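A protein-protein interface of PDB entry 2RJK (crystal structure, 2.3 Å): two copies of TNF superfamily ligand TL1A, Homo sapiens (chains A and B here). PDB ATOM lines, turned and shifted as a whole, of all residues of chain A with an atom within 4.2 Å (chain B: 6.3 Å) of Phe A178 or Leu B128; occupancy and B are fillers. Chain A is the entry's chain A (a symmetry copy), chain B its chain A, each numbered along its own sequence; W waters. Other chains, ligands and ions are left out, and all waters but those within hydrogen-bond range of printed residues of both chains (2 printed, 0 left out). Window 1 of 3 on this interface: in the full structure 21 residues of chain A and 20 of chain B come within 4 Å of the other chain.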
ATOM      1  N   HIS A  31     -21.351   1.653  20.732  1.00  0.00           N
ATOM      2  CA  HIS A  31     -20.650   0.527  20.179  1.00  0.00           C
ATOM      3  C   HIS A  31     -19.304   0.991  19.650  1.00  0.00           C
ATOM      4  O   HIS A  31     -19.268   1.774  18.733  1.00  0.00           O
ATOM      5  CB  HIS A  31     -21.466  -0.117  19.026  1.00  0.00           C
ATOM      6  CG  HIS A  31     -20.851  -1.366  18.462  1.00  0.00           C
ATOM      7  ND1 HIS A  31     -20.812  -2.566  19.149  1.00  0.00           N
ATOM      8  CD2 HIS A  31     -20.279  -1.608  17.251  1.00  0.00           C
ATOM      9  CE1 HIS A  31     -20.240  -3.491  18.381  1.00  0.00           C
ATOM     10  NE2 HIS A  31     -19.913  -2.934  17.225  1.00  0.00           N
ATOM     11  N   LEU A  32     -18.210   0.435  20.165  1.00  0.00           N
ATOM     12  CA  LEU A  32     -16.848   0.771  19.701  1.00  0.00           C
ATOM     13  C   LEU A  32     -16.191  -0.430  19.026  1.00  0.00           C
ATOM     14  O   LEU A  32     -16.469  -1.580  19.376  1.00  0.00           O
ATOM     15  CB  LEU A  32     -15.999   1.220  20.908  1.00  0.00           C
ATOM     16  CG  LEU A  32     -16.710   2.210  21.868  1.00  0.00           C
ATOM     17  CD1 LEU A  32     -15.856   2.489  23.043  1.00  0.00           C
ATOM     18  CD2 LEU A  32     -17.156   3.558  21.225  1.00  0.00           C
ATOM     19  N   THR A  33     -15.319  -0.152  18.062  1.00  0.00           N
ATOM     20  CA  THR A  33     -14.736  -1.158  17.224  1.00  0.00           C
ATOM     21  C   THR A  33     -13.223  -1.002  17.254  1.00  0.00           C
ATOM     22  O   THR A  33     -12.680   0.078  17.536  1.00  0.00           O
ATOM     23  CB  THR A  33     -15.358  -1.058  15.799  1.00  0.00           C
ATOM     24  OG1 THR A  33     -15.057   0.230  15.236  1.00  0.00           O
ATOM     25  CG2 THR A  33     -16.888  -1.113  15.983  1.00  0.00           C
ATOM     26  N   TRP A  52     -10.003   2.550  20.955  1.00  0.00           N
ATOM     27  CA  TRP A  52     -11.113   2.114  20.112  1.00  0.00           C
ATOM     28  C   TRP A  52     -11.462   3.170  19.088  1.00  0.00           C
ATOM     29  O   TRP A  52     -11.197   4.356  19.296  1.00  0.00           O
ATOM     30  CB  TRP A  52     -12.383   1.925  21.007  1.00  0.00           C
ATOM     31  CG  TRP A  52     -12.175   0.867  22.025  1.00  0.00           C
ATOM     32  CD1 TRP A  52     -11.827   1.023  23.341  1.00  0.00           C
ATOM     33  CD2 TRP A  52     -12.283  -0.546  21.790  1.00  0.00           C
ATOM     34  NE1 TRP A  52     -11.671  -0.229  23.937  1.00  0.00           N
ATOM     35  CE2 TRP A  52     -11.982  -1.199  23.007  1.00  0.00           C
ATOM     36  CE3 TRP A  52     -12.633  -1.325  20.655  1.00  0.00           C
ATOM     37  CZ2 TRP A  52     -11.993  -2.603  23.126  1.00  0.00           C
ATOM     38  CZ3 TRP A  52     -12.635  -2.722  20.766  1.00  0.00           C
ATOM     39  CH2 TRP A  52     -12.328  -3.344  22.004  1.00  0.00           C
ATOM     40  N   TYR A  83     -20.598  -5.232  26.925  1.00  0.00           N
ATOM     41  CA  TYR A  83     -20.101  -6.416  26.232  1.00  0.00           C
ATOM     42  C   TYR A  83     -18.865  -6.102  25.426  1.00  0.00           C
ATOM     43  O   TYR A  83     -18.617  -4.946  25.065  1.00  0.00           O
ATOM     44  CB  TYR A  83     -21.197  -6.963  25.291  1.00  0.00           C
ATOM     45  CG  TYR A  83     -21.526  -5.979  24.202  1.00  0.00           C
ATOM     46  CD1 TYR A  83     -20.730  -5.896  23.058  1.00  0.00           C
ATOM     47  CD2 TYR A  83     -22.606  -5.099  24.318  1.00  0.00           C
ATOM     48  CE1 TYR A  83     -20.995  -4.978  22.079  1.00  0.00           C
ATOM     49  CE2 TYR A  83     -22.864  -4.150  23.329  1.00  0.00           C
ATOM     50  CZ  TYR A  83     -22.076  -4.107  22.206  1.00  0.00           C
ATOM     51  OH  TYR A  83     -22.368  -3.204  21.190  1.00  0.00           O
ATOM     52  N   SER A  84     -18.095  -7.142  25.125  1.00  0.00           N
ATOM     53  CA  SER A  84     -16.923  -7.009  24.296  1.00  0.00           C
ATOM     54  C   SER A  84     -16.567  -8.347  23.693  1.00  0.00           C
ATOM     55  O   SER A  84     -16.672  -9.382  24.337  1.00  0.00           O
ATOM     56  CB  SER A  84     -15.719  -6.554  25.142  1.00  0.00           C
ATOM     57  OG  SER A  84     -14.542  -6.458  24.335  1.00  0.00           O
ATOM     58  N   GLN A  85     -16.132  -8.323  22.443  1.00  0.00           N
ATOM     59  CA  GLN A  85     -15.410  -9.440  21.923  1.00  0.00           C
ATOM     60  C   GLN A  85     -14.011  -8.961  21.495  1.00  0.00           C
ATOM     61  O   GLN A  85     -13.842  -7.897  20.856  1.00  0.00           O
ATOM     62  CB  GLN A  85     -16.134 -10.058  20.727  1.00  0.00           C
ATOM     63  CG  GLN A  85     -15.244 -11.075  20.042  1.00  0.00           C
ATOM     64  CD  GLN A  85     -15.941 -11.793  18.964  1.00  0.00           C
ATOM     65  OE1 GLN A  85     -16.560 -12.803  19.227  1.00  0.00           O
ATOM     66  NE2 GLN A  85     -15.826 -11.314  17.716  1.00  0.00           N
ATOM     67  N   TYR A 146     -15.687 -13.697  23.815  1.00  0.00           N
ATOM     68  CA  TYR A 146     -16.832 -12.783  23.928  1.00  0.00           C
ATOM     69  C   TYR A 146     -17.321 -12.755  25.369  1.00  0.00           C
ATOM     70  O   TYR A 146     -17.370 -13.772  26.012  1.00  0.00           O
ATOM     71  CB  TYR A 146     -17.976 -13.204  23.007  1.00  0.00           C
ATOM     72  CG  TYR A 146     -19.182 -12.314  23.130  1.00  0.00           C
ATOM     73  CD1 TYR A 146     -19.380 -11.256  22.248  1.00  0.00           C
ATOM     74  CD2 TYR A 146     -20.073 -12.471  24.176  1.00  0.00           C
ATOM     75  CE1 TYR A 146     -20.481 -10.431  22.358  1.00  0.00           C
ATOM     76  CE2 TYR A 146     -21.167 -11.605  24.329  1.00  0.00           C
ATOM     77  CZ  TYR A 146     -21.366 -10.583  23.405  1.00  0.00           C
ATOM     78  OH  TYR A 146     -22.419  -9.693  23.523  1.00  0.00           O
ATOM     79  N   ASP A 175     -15.650  -5.819  12.798  1.00  0.00           N
ATOM     80  CA  ASP A 175     -16.675  -6.798  13.192  1.00  0.00           C
ATOM     81  C   ASP A 175     -16.044  -7.900  14.042  1.00  0.00           C
ATOM     82  O   ASP A 175     -16.741  -8.791  14.516  1.00  0.00           O
ATOM     83  CB  ASP A 175     -17.418  -7.379  11.961  1.00  0.00           C
ATOM     84  CG  ASP A 175     -16.472  -8.028  10.942  1.00  0.00           C
ATOM     85  OD1 ASP A 175     -15.257  -7.759  10.991  1.00  0.00           O
ATOM     86  OD2 ASP A 175     -16.932  -8.817  10.083  1.00  0.00           O
ATOM     87  N   LYS A 176     -14.721  -7.856  14.224  1.00  0.00           N
ATOM     88  CA  LYS A 176     -14.067  -8.920  14.997  1.00  0.00           C
ATOM     89  C   LYS A 176     -13.743  -8.564  16.435  1.00  0.00           C
ATOM     90  O   LYS A 176     -13.742  -9.441  17.318  1.00  0.00           O
ATOM     91  CB  LYS A 176     -12.808  -9.435  14.310  1.00  0.00           C
ATOM     92  CG  LYS A 176     -13.134 -10.137  13.002  1.00  0.00           C
ATOM     93  CD  LYS A 176     -12.040 -10.989  12.496  1.00  0.00           C
ATOM     94  CE  LYS A 176     -11.043 -10.225  11.664  1.00  0.00           C
ATOM     95  NZ  LYS A 176     -10.045 -11.222  11.134  1.00  0.00           N
ATOM     96  N   THR A 177     -13.471  -7.292  16.685  1.00  0.00           N
ATOM     97  CA  THR A 177     -13.105  -6.900  18.036  1.00  0.00           C
ATOM     98  C   THR A 177     -13.866  -5.603  18.273  1.00  0.00           C
ATOM     99  O   THR A 177     -13.773  -4.685  17.451  1.00  0.00           O
ATOM    100  CB  THR A 177     -11.611  -6.642  18.121  1.00  0.00           C
ATOM    101  OG1 THR A 177     -10.938  -7.865  17.935  1.00  0.00           O
ATOM    102  CG2 THR A 177     -11.204  -6.092  19.459  1.00  0.00           C
ATOM    103  N   PHE A 178     -14.615  -5.528  19.369  1.00  0.00           N
ATOM    104  CA  PHE A 178     -15.546  -4.425  19.606  1.00  0.00           C
ATOM    105  C   PHE A 178     -15.896  -4.449  21.094  1.00  0.00           C
ATOM    106  O   PHE A 178     -15.546  -5.395  21.815  1.00  0.00           O
ATOM    107  CB  PHE A 178     -16.831  -4.567  18.758  1.00  0.00           C
ATOM    108  CG  PHE A 178     -17.472  -5.956  18.847  1.00  0.00           C
ATOM    109  CD1 PHE A 178     -18.236  -6.308  19.936  1.00  0.00           C
ATOM    110  CD2 PHE A 178     -17.252  -6.906  17.865  1.00  0.00           C
ATOM    111  CE1 PHE A 178     -18.790  -7.586  20.023  1.00  0.00           C
ATOM    112  CE2 PHE A 178     -17.824  -8.180  17.943  1.00  0.00           C
ATOM    113  CZ  PHE A 178     -18.601  -8.494  19.043  1.00  0.00           C
ATOM    114  N   PHE A 179     -16.574  -3.394  21.539  1.00  0.00           N
ATOM    115  CA  PHE A 179     -16.809  -3.135  22.968  1.00  0.00           C
ATOM    116  C   PHE A 179     -18.006  -2.197  22.958  1.00  0.00           C
ATOM    117  O   PHE A 179     -17.971  -1.178  22.287  1.00  0.00           O
ATOM    118  CB  PHE A 179     -15.533  -2.464  23.541  1.00  0.00           C
ATOM    119  CG  PHE A 179     -15.672  -1.786  24.913  1.00  0.00           C
ATOM    120  CD1 PHE A 179     -16.397  -2.359  25.956  1.00  0.00           C
ATOM    121  CD2 PHE A 179     -14.948  -0.601  25.185  1.00  0.00           C
ATOM    122  CE1 PHE A 179     -16.457  -1.740  27.238  1.00  0.00           C
ATOM    123  CE2 PHE A 179     -15.000   0.028  26.476  1.00  0.00           C
ATOM    124  CZ  PHE A 179     -15.772  -0.544  27.491  1.00  0.00           C
ATOM    125  N   ILE B  82     -28.392  -7.613  18.697  1.00  0.00           N
ATOM    126  CA  ILE B  82     -28.499  -8.715  17.761  1.00  0.00           C
ATOM    127  C   ILE B  82     -27.520  -9.801  18.204  1.00  0.00           C
ATOM    128  O   ILE B  82     -26.404  -9.470  18.611  1.00  0.00           O
ATOM    129  CB  ILE B  82     -28.000  -8.186  16.393  1.00  0.00           C
ATOM    130  CG1 ILE B  82     -28.964  -7.126  15.886  1.00  0.00           C
ATOM    131  CG2 ILE B  82     -27.918  -9.278  15.409  1.00  0.00           C
ATOM    132  CD1 ILE B  82     -28.469  -6.502  14.636  1.00  0.00           C
ATOM    133  N   TYR B  83     -27.885 -11.081  18.073  1.00  0.00           N
ATOM    134  CA  TYR B  83     -26.987 -12.115  18.576  1.00  0.00           C
ATOM    135  C   TYR B  83     -27.212 -13.429  17.871  1.00  0.00           C
ATOM    136  O   TYR B  83     -28.285 -13.672  17.306  1.00  0.00           O
ATOM    137  CB  TYR B  83     -27.215 -12.305  20.092  1.00  0.00           C
ATOM    138  CG  TYR B  83     -28.601 -12.816  20.378  1.00  0.00           C
ATOM    139  CD1 TYR B  83     -28.893 -14.176  20.268  1.00  0.00           C
ATOM    140  CD2 TYR B  83     -29.639 -11.945  20.723  1.00  0.00           C
ATOM    141  CE1 TYR B  83     -30.159 -14.647  20.486  1.00  0.00           C
ATOM    142  CE2 TYR B  83     -30.934 -12.423  20.926  1.00  0.00           C
ATOM    143  CZ  TYR B  83     -31.185 -13.769  20.830  1.00  0.00           C
ATOM    144  OH  TYR B  83     -32.461 -14.255  21.093  1.00  0.00           O
ATOM    145  N   SER B  84     -26.202 -14.289  17.920  1.00  0.00           N
ATOM    146  CA  SER B  84     -26.298 -15.614  17.358  1.00  0.00           C
ATOM    147  C   SER B  84     -25.272 -16.518  17.998  1.00  0.00           C
ATOM    148  O   SER B  84     -24.149 -16.115  18.267  1.00  0.00           O
ATOM    149  CB  SER B  84     -25.996 -15.577  15.848  1.00  0.00           C
ATOM    150  OG  SER B  84     -26.051 -16.892  15.290  1.00  0.00           O
ATOM    151  N   VAL B 112     -18.512 -17.737  11.866  1.00  0.00           N
ATOM    152  CA  VAL B 112     -19.859 -17.160  11.772  1.00  0.00           C
ATOM    153  C   VAL B 112     -19.807 -15.651  11.518  1.00  0.00           C
ATOM    154  O   VAL B 112     -18.987 -14.939  12.109  1.00  0.00           O
ATOM    155  CB  VAL B 112     -20.583 -17.301  13.104  1.00  0.00           C
ATOM    156  CG1 VAL B 112     -22.021 -16.785  12.953  1.00  0.00           C
ATOM    157  CG2 VAL B 112     -20.541 -18.688  13.517  1.00  0.00           C
ATOM    158  N   VAL B 113     -20.697 -15.158  10.676  1.00  0.00           N
ATOM    159  CA  VAL B 113     -20.780 -13.739  10.368  1.00  0.00           C
ATOM    160  C   VAL B 113     -22.248 -13.353  10.359  1.00  0.00           C
ATOM    161  O   VAL B 113     -23.083 -14.057   9.787  1.00  0.00           O
ATOM    162  CB  VAL B 113     -20.299 -13.422   8.917  1.00  0.00           C
ATOM    163  CG1 VAL B 113     -20.357 -11.916   8.683  1.00  0.00           C
ATOM    164  CG2 VAL B 113     -18.904 -13.896   8.696  1.00  0.00           C
ATOM    165  N   ILE B 114     -22.571 -12.245  10.996  1.00  0.00           N
ATOM    166  CA  ILE B 114     -23.902 -11.702  10.928  1.00  0.00           C
ATOM    167  C   ILE B 114     -23.828 -10.480  10.041  1.00  0.00           C
ATOM    168  O   ILE B 114     -22.989  -9.601  10.249  1.00  0.00           O
ATOM    169  CB  ILE B 114     -24.406 -11.308  12.335  1.00  0.00           C
ATOM    170  CG1 ILE B 114     -24.448 -12.558  13.262  1.00  0.00           C
ATOM    171  CG2 ILE B 114     -25.814 -10.680  12.238  1.00  0.00           C
ATOM    172  CD1 ILE B 114     -25.128 -12.238  14.567  1.00  0.00           C
ATOM    173  N   THR B 115     -24.737 -10.402   9.080  1.00  0.00           N
ATOM    174  CA  THR B 115     -24.604  -9.478   7.974  1.00  0.00           C
ATOM    175  C   THR B 115     -25.887  -8.693   7.863  1.00  0.00           C
ATOM    176  O   THR B 115     -26.964  -9.189   8.155  1.00  0.00           O
ATOM    177  CB  THR B 115     -24.401 -10.269   6.639  1.00  0.00           C
ATOM    178  OG1 THR B 115     -23.144 -10.963   6.674  1.00  0.00           O
ATOM    179  CG2 THR B 115     -24.420  -9.342   5.433  1.00  0.00           C
ATOM    180  N   THR B 125     -23.154  -5.463   4.681  1.00  0.00           N
ATOM    181  CA  THR B 125     -22.218  -5.010   5.701  1.00  0.00           C
ATOM    182  C   THR B 125     -22.066  -6.099   6.763  1.00  0.00           C
ATOM    183  O   THR B 125     -23.052  -6.572   7.300  1.00  0.00           O
ATOM    184  CB  THR B 125     -22.685  -3.673   6.292  1.00  0.00           C
ATOM    185  OG1 THR B 125     -22.653  -2.684   5.258  1.00  0.00           O
ATOM    186  CG2 THR B 125     -21.794  -3.187   7.488  1.00  0.00           C
ATOM    187  N   GLN B 126     -20.839  -6.530   7.032  1.00  0.00           N
ATOM    188  CA  GLN B 126     -20.606  -7.431   8.151  1.00  0.00           C
ATOM    189  C   GLN B 126     -20.692  -6.679   9.467  1.00  0.00           C
ATOM    190  O   GLN B 126     -19.939  -5.722   9.725  1.00  0.00           O
ATOM    191  CB  GLN B 126     -19.267  -8.167   8.009  1.00  0.00           C
ATOM    192  CG  GLN B 126     -19.226  -9.077   6.767  1.00  0.00           C
ATOM    193  CD  GLN B 126     -17.854  -9.751   6.529  1.00  0.00           C
ATOM    194  OE1 GLN B 126     -17.578 -10.182   5.421  1.00  0.00           O
ATOM    195  NE2 GLN B 126     -17.001  -9.831   7.565  1.00  0.00           N
ATOM    196  N   LEU B 127     -21.629  -7.118  10.293  1.00  0.00           N
ATOM    197  CA  LEU B 127     -21.784  -6.561  11.626  1.00  0.00           C
ATOM    198  C   LEU B 127     -20.864  -7.230  12.652  1.00  0.00           C
ATOM    199  O   LEU B 127     -20.153  -6.554  13.391  1.00  0.00           O
ATOM    200  CB  LEU B 127     -23.264  -6.661  12.034  1.00  0.00           C
ATOM    201  CG  LEU B 127     -24.289  -5.993  11.093  1.00  0.00           C
ATOM    202  CD1 LEU B 127     -25.617  -6.130  11.710  1.00  0.00           C
ATOM    203  CD2 LEU B 127     -23.992  -4.483  10.855  1.00  0.00           C
ATOM    204  N   LEU B 128     -20.809  -8.560  12.647  1.00  0.00           N
ATOM    205  CA  LEU B 128     -20.153  -9.324  13.728  1.00  0.00           C
ATOM    206  C   LEU B 128     -19.497 -10.475  13.070  1.00  0.00           C
ATOM    207  O   LEU B 128     -20.120 -11.085  12.236  1.00  0.00           O
ATOM    208  CB  LEU B 128     -21.231  -9.894  14.653  1.00  0.00           C
ATOM    209  CG  LEU B 128     -21.952  -8.839  15.496  1.00  0.00           C
ATOM    210  CD1 LEU B 128     -23.193  -9.353  16.211  1.00  0.00           C
ATOM    211  CD2 LEU B 128     -20.953  -8.236  16.499  1.00  0.00           C
ATOM    212  N   MET B 129     -18.253 -10.778  13.425  1.00  0.00           N
ATOM    213  CA  MET B 129     -17.628 -11.982  12.910  1.00  0.00           C
ATOM    214  C   MET B 129     -16.923 -12.760  14.038  1.00  0.00           C
ATOM    215  O   MET B 129     -16.183 -12.187  14.851  1.00  0.00           O
ATOM    216  CB  MET B 129     -16.610 -11.660  11.786  1.00  0.00           C
ATOM    217  CG  MET B 129     -15.785 -12.873  11.378  1.00  0.00           C
ATOM    218  SD  MET B 129     -14.639 -12.571   9.989  1.00  0.00           S
ATOM    219  CE  MET B 129     -15.842 -12.253   8.712  1.00  0.00           C
ATOM    220  N   GLY B 130     -17.214 -14.050  14.117  1.00  0.00           N
ATOM    221  CA  GLY B 130     -16.556 -14.961  15.062  1.00  0.00           C
ATOM    222  C   GLY B 130     -15.840 -16.040  14.291  1.00  0.00           C
ATOM    223  O   GLY B 130     -16.440 -16.853  13.571  1.00  0.00           O
ATOM    224  N   LEU B 147     -21.939 -14.658  19.391  1.00  0.00           N
ATOM    225  CA  LEU B 147     -21.699 -13.227  19.081  1.00  0.00           C
ATOM    226  C   LEU B 147     -22.958 -12.477  19.365  1.00  0.00           C
ATOM    227  O   LEU B 147     -24.045 -12.951  19.015  1.00  0.00           O
ATOM    228  CB  LEU B 147     -21.541 -13.041  17.553  1.00  0.00           C
ATOM    229  CG  LEU B 147     -20.420 -13.686  16.770  1.00  0.00           C
ATOM    230  CD1 LEU B 147     -20.757 -13.825  15.270  1.00  0.00           C
ATOM    231  CD2 LEU B 147     -19.192 -12.812  17.001  1.00  0.00           C
ATOM    232  N   GLY B 148     -22.834 -11.298  19.966  1.00  0.00           N
ATOM    233  CA  GLY B 148     -23.964 -10.368  20.135  1.00  0.00           C
ATOM    234  C   GLY B 148     -23.452  -8.929  20.252  1.00  0.00           C
ATOM    235  O   GLY B 148     -22.403  -8.695  20.872  1.00  0.00           O
ATOM    236  N   ALA B 149     -24.163  -7.961  19.657  1.00  0.00           N
ATOM    237  CA  ALA B 149     -23.848  -6.525  19.881  1.00  0.00           C
ATOM    238  C   ALA B 149     -24.961  -5.624  19.446  1.00  0.00           C
ATOM    239  O   ALA B 149     -25.946  -6.091  18.862  1.00  0.00           O
ATOM    240  CB  ALA B 149     -22.514  -6.087  19.202  1.00  0.00           C
ATOM    241  N   PHE B 151     -26.461  -2.382  17.264  1.00  0.00           N
ATOM    242  CA  PHE B 151     -26.283  -1.675  15.978  1.00  0.00           C
ATOM    243  C   PHE B 151     -27.463  -0.783  15.692  1.00  0.00           C
ATOM    244  O   PHE B 151     -28.591  -1.085  16.107  1.00  0.00           O
ATOM    245  CB  PHE B 151     -26.125  -2.668  14.831  1.00  0.00           C
ATOM    246  CG  PHE B 151     -24.918  -3.559  14.992  1.00  0.00           C
ATOM    247  CD1 PHE B 151     -23.695  -3.146  14.557  1.00  0.00           C
ATOM    248  CD2 PHE B 151     -25.022  -4.813  15.599  1.00  0.00           C
ATOM    249  CE1 PHE B 151     -22.533  -3.951  14.738  1.00  0.00           C
ATOM    250  CE2 PHE B 151     -23.908  -5.614  15.753  1.00  0.00           C
ATOM    251  CZ  PHE B 151     -22.651  -5.165  15.352  1.00  0.00           C
HETATM  252  O   HOH W   1     -18.876  -4.286  14.954  1.00  0.00           O
HETATM  253  O   HOH W   2     -14.093  -9.758   9.664  1.00  0.00           O
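O of Asp A175 sits at hydrogen-bond distance from N of Met B129 (2.7 Å). The side-chain amide nitrogen of Gln B126 is in hydrogen-bond range of the side-chain carboxylate of Asp A175 (2.7 Å). The side-chain hydroxyl of Tyr A146 lies within hydrogen-bond range of the backbone carbonyl oxygen of Gly B148, 2.8 Å away. The backbone carbonyl oxygen (O) of Met B129 is in hydrogen-bond range of the side-chain amide nitrogen (NE2) of Gln A85 (3.0 Å).
The backbone NH (N) of Ser B84 is in hydrogen-bond range of the backbone carbonyl oxygen (O) of Leu B147 (2.8 Å). The side-chain amide nitrogen of Gln A85 sits at hydrogen-bond distance from the backbone carbonyl oxygen of Lys A176 (2.8 Å). N of Ile B114 lies within hydrogen-bond range of O of Leu B128 (3.0 Å). The side-chain hydroxyl (OG) of Ser A84 lies within hydrogen-bond range of the backbone carbonyl oxygen (O) of Phe A178, at 2.9 Å. The backbone carbonyl oxygen (O) of Gln A85 sits at hydrogen-bond distance from the backbone NH (N) of Phe A178. A ring nitrogen (ND1) of His A31 sits at hydrogen-bond distance from the side-chain hydroxyl (OH) of Tyr A83 (2.6 Å).
CE1 of His A31 touches CB of Ala B149, 3.5 Å away. His A31 touches Phe B151 (NE2 to CE1, 3.8 Å). O of Gly B148 touches CD1 of Tyr A83, at 3.9 Å. Ala B149 touches Tyr A83 (CB to CE1, 3.4 Å). Leu B147 touches Gln A85. Leu B127 touches Asp A175 (O to CB, 3.2 Å). O of Asp A175 touches C of Leu B128 (3.5 Å). O of Met B129 touches CA of Lys A176, 3.9 Å away. Phe A178 touches Leu B128 (CE2 to CD2, 3.4 Å). Phe A178 touches Gly B148 (CE1 to O, 3.9 Å).
Phe A178 touches just these residues of chain B: Leu B128 (3.4 Å) and Gly B148 (3.9 Å). Thr B125 touches none of the printed residues of chain A. Of the printed residues of chain A, Gln B126 touches Asp A175. Leu B128 touches just these residues of chain A: Asp A175 (3.5 Å) and Phe A178 (3.4 Å). Of the printed residues of chain A, Ala B149 touches His A31 and Tyr A83. Of the printed residues of chain A, Phe B151 touches His A31 (3.8 Å). The nearest residue of chain B that does not touch Phe A178 is Ala B149 (4.1 Å). The nearest printed residue of chain A that does not touch Leu B128 is His A31 (5.2 Å).
Printed residues of chain A that touch a printed residue of chain B: His A31, Tyr A83, Gln A85, Tyr A146, Asp A175, Lys A176 and Phe A178. Hydrophobic or aromatic side chains of chain A within 4 Å of the printed part of chain B: His A31, Tyr A83, Tyr A146 and Phe A178. Printed residues of chain B that touch a printed residue of chain A: Gln B126, Leu B127, Leu B128, Met B129, Leu B147, Gly B148, Ala B149 and Phe B151. Among the printed residues, no Asp or Glu carboxylate lies within 4 Å of a Lys or Arg side-chain nitrogen of the other chain.
Positions printed for both chains: 83 and 84. Of the 14 pairs that touch across the chains among the printed residues, none has its exchanged pair printed and touching as well.
Water W2 lies within hydrogen-bond range of OD1 of Asp A175 and SD of Met B129. Water W1 lies within hydrogen-bond range of a ring nitrogen (NE2) of His A31 and the backbone carbonyl oxygen of Leu B127.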
